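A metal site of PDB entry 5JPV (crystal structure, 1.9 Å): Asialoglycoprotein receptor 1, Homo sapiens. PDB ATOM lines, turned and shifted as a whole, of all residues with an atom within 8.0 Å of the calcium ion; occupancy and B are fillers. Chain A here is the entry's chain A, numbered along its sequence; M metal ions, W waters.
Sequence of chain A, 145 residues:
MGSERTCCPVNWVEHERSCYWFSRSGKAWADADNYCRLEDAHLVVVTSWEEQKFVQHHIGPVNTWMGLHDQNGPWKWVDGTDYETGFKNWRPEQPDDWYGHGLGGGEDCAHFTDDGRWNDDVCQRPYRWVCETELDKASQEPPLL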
ATOM      1  N   HIS A  15       2.794   1.447  -7.853  1.00  0.00           N
ATOM      2  CA  HIS A  15       3.324   1.893  -9.116  1.00  0.00           C
ATOM      3  C   HIS A  15       3.009   3.366  -9.342  1.00  0.00           C
ATOM      4  O   HIS A  15       1.842   3.758  -9.363  1.00  0.00           O
ATOM      5  CB  HIS A  15       2.769   1.053 -10.270  1.00  0.00           C
ATOM      6  CG  HIS A  15       3.176   1.550 -11.629  1.00  0.00           C
ATOM      7  ND1 HIS A  15       4.364   1.176 -12.224  1.00  0.00           N
ATOM      8  CD2 HIS A  15       2.566   2.395 -12.489  1.00  0.00           C
ATOM      9  CE1 HIS A  15       4.465   1.771 -13.401  1.00  0.00           C
ATOM     10  NE2 HIS A  15       3.379   2.520 -13.581  1.00  0.00           N
ATOM     11  N   GLU A  16       4.069   4.163  -9.488  1.00  0.00           N
ATOM     12  CA  GLU A  16       3.954   5.590  -9.809  1.00  0.00           C
ATOM     13  C   GLU A  16       2.874   6.302  -9.000  1.00  0.00           C
ATOM     14  O   GLU A  16       1.918   6.853  -9.554  1.00  0.00           O
ATOM     15  CB  GLU A  16       3.734   5.764 -11.323  1.00  0.00           C
ATOM     16  CG  GLU A  16       4.532   6.914 -11.950  1.00  0.00           C
ATOM     17  CD  GLU A  16       6.036   6.684 -11.925  1.00  0.00           C
ATOM     18  OE1 GLU A  16       6.533   5.710 -12.537  1.00  0.00           O
ATOM     19  OE2 GLU A  16       6.737   7.497 -11.279  1.00  0.00           O
ATOM     20  N   SER A  18       0.492   5.262  -7.167  1.00  0.00           N
ATOM     21  CA  SER A  18      -0.784   4.536  -7.008  1.00  0.00           C
ATOM     22  C   SER A  18      -0.580   3.139  -6.458  1.00  0.00           C
ATOM     23  O   SER A  18       0.487   2.539  -6.637  1.00  0.00           O
ATOM     24  CB  SER A  18      -1.515   4.443  -8.353  1.00  0.00           C
ATOM     25  OG  SER A  18      -2.347   5.566  -8.580  1.00  0.00           O
ATOM     26  N   CYS A  19      -1.622   2.607  -5.811  1.00  0.00           N
ATOM     27  CA  CYS A  19      -1.660   1.213  -5.362  1.00  0.00           C
ATOM     28  C   CYS A  19      -2.681   0.450  -6.176  1.00  0.00           C
ATOM     29  O   CYS A  19      -3.794   0.931  -6.375  1.00  0.00           O
ATOM     30  CB  CYS A  19      -2.101   1.150  -3.903  1.00  0.00           C
ATOM     31  SG  CYS A  19      -1.090   2.133  -2.813  1.00  0.00           S
ATOM     32  N   TYR A  20      -2.325  -0.759  -6.617  1.00  0.00           N
ATOM     33  CA  TYR A  20      -3.236  -1.575  -7.428  1.00  0.00           C
ATOM     34  C   TYR A  20      -3.476  -2.947  -6.814  1.00  0.00           C
ATOM     35  O   TYR A  20      -2.556  -3.576  -6.275  1.00  0.00           O
ATOM     36  CB  TYR A  20      -2.679  -1.779  -8.843  1.00  0.00           C
ATOM     37  CG  TYR A  20      -2.365  -0.490  -9.577  1.00  0.00           C
ATOM     38  CD1 TYR A  20      -1.195   0.228  -9.287  1.00  0.00           C
ATOM     39  CD2 TYR A  20      -3.235   0.008 -10.541  1.00  0.00           C
ATOM     40  CE1 TYR A  20      -0.914   1.414  -9.949  1.00  0.00           C
ATOM     41  CE2 TYR A  20      -2.951   1.208 -11.220  1.00  0.00           C
ATOM     42  CZ  TYR A  20      -1.792   1.900 -10.914  1.00  0.00           C
ATOM     43  OH  TYR A  20      -1.491   3.064 -11.555  1.00  0.00           O
ATOM     44  N   HIS A  42     -11.097   2.493  -6.227  1.00  0.00           N
ATOM     45  CA  HIS A  42     -12.009   2.586  -7.374  1.00  0.00           C
ATOM     46  C   HIS A  42     -11.477   1.658  -8.457  1.00  0.00           C
ATOM     47  O   HIS A  42     -10.290   1.361  -8.474  1.00  0.00           O
ATOM     48  CB  HIS A  42     -12.066   4.033  -7.878  1.00  0.00           C
ATOM     49  CG  HIS A  42     -10.739   4.605  -8.254  1.00  0.00           C
ATOM     50  ND1 HIS A  42     -10.114   4.312  -9.453  1.00  0.00           N
ATOM     51  CD2 HIS A  42      -9.900   5.440  -7.595  1.00  0.00           C
ATOM     52  CE1 HIS A  42      -8.943   4.931  -9.509  1.00  0.00           C
ATOM     53  NE2 HIS A  42      -8.801   5.639  -8.393  1.00  0.00           N
ATOM     54  N   LEU A  43     -12.353   1.195  -9.354  1.00  0.00           N
ATOM     55  CA  LEU A  43     -11.876   0.435 -10.515  1.00  0.00           C
ATOM     56  C   LEU A  43     -10.800   1.254 -11.246  1.00  0.00           C
ATOM     57  O   LEU A  43     -10.914   2.466 -11.366  1.00  0.00           O
ATOM     58  CB  LEU A  43     -13.028   0.106 -11.463  1.00  0.00           C
ATOM     59  CG  LEU A  43     -13.974  -1.037 -11.066  1.00  0.00           C
ATOM     60  CD1 LEU A  43     -15.219  -0.995 -11.938  1.00  0.00           C
ATOM     61  CD2 LEU A  43     -13.273  -2.402 -11.194  1.00  0.00           C
ATOM     62  N   VAL A  44      -9.775   0.565 -11.738  1.00  0.00           N
ATOM     63  CA  VAL A  44      -8.607   1.245 -12.317  1.00  0.00           C
ATOM     64  C   VAL A  44      -8.982   2.322 -13.351  1.00  0.00           C
ATOM     65  O   VAL A  44      -9.851   2.108 -14.197  1.00  0.00           O
ATOM     66  CB  VAL A  44      -7.555   0.219 -12.866  1.00  0.00           C
ATOM     67  CG1 VAL A  44      -8.079  -0.533 -14.099  1.00  0.00           C
ATOM     68  CG2 VAL A  44      -6.195   0.882 -13.108  1.00  0.00           C
ATOM     69  N   VAL A  45      -8.344   3.478 -13.233  1.00  0.00           N
ATOM     70  CA  VAL A  45      -8.507   4.590 -14.176  1.00  0.00           C
ATOM     71  C   VAL A  45      -7.156   4.747 -14.864  1.00  0.00           C
ATOM     72  O   VAL A  45      -6.150   4.997 -14.210  1.00  0.00           O
ATOM     73  CB  VAL A  45      -8.949   5.891 -13.452  1.00  0.00           C
ATOM     74  CG1 VAL A  45      -8.879   7.123 -14.387  1.00  0.00           C
ATOM     75  CG2 VAL A  45     -10.386   5.744 -12.908  1.00  0.00           C
ATOM     76  N   VAL A  46      -7.129   4.532 -16.178  1.00  0.00           N
ATOM     77  CA  VAL A  46      -5.859   4.496 -16.923  1.00  0.00           C
ATOM     78  C   VAL A  46      -5.652   5.821 -17.650  1.00  0.00           C
ATOM     79  O   VAL A  46      -6.476   6.215 -18.469  1.00  0.00           O
ATOM     80  CB  VAL A  46      -5.830   3.320 -17.940  1.00  0.00           C
ATOM     81  CG1 VAL A  46      -4.497   3.286 -18.697  1.00  0.00           C
ATOM     82  CG2 VAL A  46      -6.045   1.992 -17.217  1.00  0.00           C
ATOM     83  N   THR A  47      -4.548   6.521 -17.357  1.00  0.00           N
ATOM     84  CA  THR A  47      -4.358   7.859 -17.938  1.00  0.00           C
ATOM     85  C   THR A  47      -3.063   8.041 -18.746  1.00  0.00           C
ATOM     86  O   THR A  47      -2.761   9.151 -19.177  1.00  0.00           O
ATOM     87  CB  THR A  47      -4.439   8.977 -16.867  1.00  0.00           C
ATOM     88  OG1 THR A  47      -3.560   8.669 -15.789  1.00  0.00           O
ATOM     89  CG2 THR A  47      -5.870   9.128 -16.355  1.00  0.00           C
ATOM     90  N   SER A  48      -2.306   6.975 -18.962  1.00  0.00           N
ATOM     91  CA  SER A  48      -1.060   7.081 -19.731  1.00  0.00           C
ATOM     92  C   SER A  48      -0.680   5.753 -20.357  1.00  0.00           C
ATOM     93  O   SER A  48      -1.180   4.696 -19.933  1.00  0.00           O
ATOM     94  CB  SER A  48       0.090   7.578 -18.853  1.00  0.00           C
ATOM     95  OG  SER A  48       0.419   6.630 -17.839  1.00  0.00           O
ATOM     96  N   GLU A  51       1.104   3.570 -17.616  1.00  0.00           N
ATOM     97  CA  GLU A  51       0.162   2.903 -16.716  1.00  0.00           C
ATOM     98  C   GLU A  51      -0.533   1.732 -17.410  1.00  0.00           C
ATOM     99  O   GLU A  51      -0.733   0.670 -16.811  1.00  0.00           O
ATOM    100  CB  GLU A  51      -0.864   3.894 -16.174  1.00  0.00           C
ATOM    101  CG  GLU A  51      -1.859   3.254 -15.206  1.00  0.00           C
ATOM    102  CD  GLU A  51      -2.777   4.247 -14.524  1.00  0.00           C
ATOM    103  OE1 GLU A  51      -3.284   3.926 -13.423  1.00  0.00           O
ATOM    104  OE2 GLU A  51      -2.997   5.351 -15.075  1.00  0.00           O
ATOM    105  N   VAL A  55      -0.405  -2.179 -16.112  1.00  0.00           N
ATOM    106  CA  VAL A  55      -1.618  -2.953 -15.881  1.00  0.00           C
ATOM    107  C   VAL A  55      -1.595  -4.208 -16.758  1.00  0.00           C
ATOM    108  O   VAL A  55      -1.771  -5.312 -16.252  1.00  0.00           O
ATOM    109  CB  VAL A  55      -2.885  -2.113 -16.086  1.00  0.00           C
ATOM    110  CG1 VAL A  55      -4.115  -2.997 -16.033  1.00  0.00           C
ATOM    111  CG2 VAL A  55      -2.977  -1.013 -15.027  1.00  0.00           C
ATOM    112  N   TRP A  77     -15.084   8.114 -16.501  1.00  0.00           N
ATOM    113  CA  TRP A  77     -14.190   7.382 -15.613  1.00  0.00           C
ATOM    114  C   TRP A  77     -14.806   7.471 -14.212  1.00  0.00           C
ATOM    115  O   TRP A  77     -15.337   8.521 -13.851  1.00  0.00           O
ATOM    116  CB  TRP A  77     -12.784   7.985 -15.616  1.00  0.00           C
ATOM    117  CG  TRP A  77     -12.027   7.724 -16.897  1.00  0.00           C
ATOM    118  CD1 TRP A  77     -11.819   8.588 -17.932  1.00  0.00           C
ATOM    119  CD2 TRP A  77     -11.390   6.496 -17.282  1.00  0.00           C
ATOM    120  NE1 TRP A  77     -11.109   7.975 -18.935  1.00  0.00           N
ATOM    121  CE2 TRP A  77     -10.835   6.691 -18.563  1.00  0.00           C
ATOM    122  CE3 TRP A  77     -11.243   5.238 -16.662  1.00  0.00           C
ATOM    123  CZ2 TRP A  77     -10.127   5.681 -19.230  1.00  0.00           C
ATOM    124  CZ3 TRP A  77     -10.532   4.244 -17.321  1.00  0.00           C
ATOM    125  CH2 TRP A  77      -9.990   4.472 -18.599  1.00  0.00           C
ATOM    126  N   ASP A  79     -13.787   7.912 -11.190  1.00  0.00           N
ATOM    127  CA  ASP A  79     -13.295   8.923 -10.245  1.00  0.00           C
ATOM    128  C   ASP A  79     -13.392  10.361 -10.758  1.00  0.00           C
ATOM    129  O   ASP A  79     -12.746  11.267 -10.209  1.00  0.00           O
ATOM    130  CB  ASP A  79     -11.844   8.615  -9.859  1.00  0.00           C
ATOM    131  CG  ASP A  79     -10.879   8.869 -10.998  1.00  0.00           C
ATOM    132  OD1 ASP A  79     -11.342   9.128 -12.136  1.00  0.00           O
ATOM    133  OD2 ASP A  79      -9.661   8.800 -10.755  1.00  0.00           O
ATOM    134  N   THR A  81     -12.285  11.628 -13.606  1.00  0.00           N
ATOM    135  CA  THR A  81     -11.292  11.983 -14.633  1.00  0.00           C
ATOM    136  C   THR A  81     -12.012  12.185 -15.969  1.00  0.00           C
ATOM    137  O   THR A  81     -12.892  11.416 -16.319  1.00  0.00           O
ATOM    138  CB  THR A  81     -10.232  10.867 -14.792  1.00  0.00           C
ATOM    139  OG1 THR A  81      -9.614  10.620 -13.526  1.00  0.00           O
ATOM    140  CG2 THR A  81      -9.150  11.267 -15.794  1.00  0.00           C
ATOM    141  N   GLU A 132      -7.755   0.434  -7.728  1.00  0.00           N
ATOM    142  CA  GLU A 132      -6.684   1.396  -7.649  1.00  0.00           C
ATOM    143  C   GLU A 132      -7.007   2.384  -6.561  1.00  0.00           C
ATOM    144  O   GLU A 132      -8.149   2.822  -6.424  1.00  0.00           O
ATOM    145  CB  GLU A 132      -6.519   2.149  -8.976  1.00  0.00           C
ATOM    146  CG  GLU A 132      -5.291   3.043  -8.984  1.00  0.00           C
ATOM    147  CD  GLU A 132      -5.177   3.923 -10.221  1.00  0.00           C
ATOM    148  OE1 GLU A 132      -6.100   3.935 -11.068  1.00  0.00           O
ATOM    149  OE2 GLU A 132      -4.126   4.609 -10.341  1.00  0.00           O
ATOM    150  N   THR A 133      -5.979   2.748  -5.791  1.00  0.00           N
ATOM    151  CA  THR A 133      -6.070   3.928  -4.938  1.00  0.00           C
ATOM    152  C   THR A 133      -4.833   4.804  -5.146  1.00  0.00           C
ATOM    153  O   THR A 133      -3.796   4.318  -5.613  1.00  0.00           O
ATOM    154  CB  THR A 133      -6.304   3.524  -3.448  1.00  0.00           C
ATOM    155  OG1 THR A 133      -6.859   4.637  -2.741  1.00  0.00           O
ATOM    156  CG2 THR A 133      -5.022   3.068  -2.795  1.00  0.00           C
ATOM    157  N   GLU A 134      -4.941   6.086  -4.842  1.00  0.00           N
ATOM    158  CA  GLU A 134      -3.818   7.011  -5.016  1.00  0.00           C
ATOM    159  C   GLU A 134      -3.167   7.323  -3.660  1.00  0.00           C
ATOM    160  O   GLU A 134      -3.865   7.484  -2.651  1.00  0.00           O
ATOM    161  CB  GLU A 134      -4.253   8.309  -5.717  1.00  0.00           C
ATOM    162  CG  GLU A 134      -4.685   8.132  -7.191  1.00  0.00           C
ATOM    163  CD  GLU A 134      -6.078   7.509  -7.346  1.00  0.00           C
ATOM    164  OE1 GLU A 134      -6.265   6.665  -8.247  1.00  0.00           O
ATOM    165  OE2 GLU A 134      -6.973   7.867  -6.552  1.00  0.00           O
HETATM  166 CA    CA M   1      -4.607   5.634 -12.551  1.00  0.00          CA
HETATM  167  O   HOH W   1      -5.980   6.949 -10.975  1.00  0.00           O
HETATM  168  O   HOH W   2      -2.600   6.713 -11.869  1.00  0.00           O
HETATM  169  O   HOH W   3      -4.725   7.739 -13.549  1.00  0.00           O
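The calcium ion is bound by the side-chain carboxylate (OE1) of Glu 51 (2.3 Å), water W3 (2.3 Å), the backbone carbonyl oxygen (O) of Val 45 (2.4 Å), water W2 (2.4 Å), water W1 (2.5 Å), the side-chain carboxylate (OE2) of Glu 132 (2.5 Å) and the side-chain carboxylate (OE1) of Glu 132 (2.7 Å).
The calcium ion has seven donor atoms within binding distance.
Slightly farther from the calcium ion lies the side-chain carboxylate (OE2) of Glu 51 (3.0 Å).
Water W3 lies within hydrogen-bond range of the side-chain hydroxyl (OG1) of Thr 47 (2.7 Å) and the side-chain carboxylate (OE2) of Glu 51 (3.3 Å).
The side-chain carboxylate (OE1) of Glu 51 sits close to the side-chain hydroxyl (OH) of Tyr 20 (2.7 Å).
The side-chain carboxylate (OE2) of Glu 51 is in hydrogen-bond range of the backbone NH (N) of Thr 47 (3.0 Å).
The side-chain hydroxyl (OG) of Ser 48 is in hydrogen-bond range of the backbone NH (N) of Glu 51, at 3.1 Å.
OE2 of Glu 132 lies close to OH of Tyr 20, 3.3 Å away.
The side-chain carboxylate (OE2) of Glu 132 lies close to the side-chain hydroxyl (OG) of Ser 18, at 2.7 Å.
N of Glu 132 sits at hydrogen-bond distance from O of His 42, 2.8 Å away.
Within 4 Å of the calcium ion: Val 45, Glu 51 and Glu 132.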
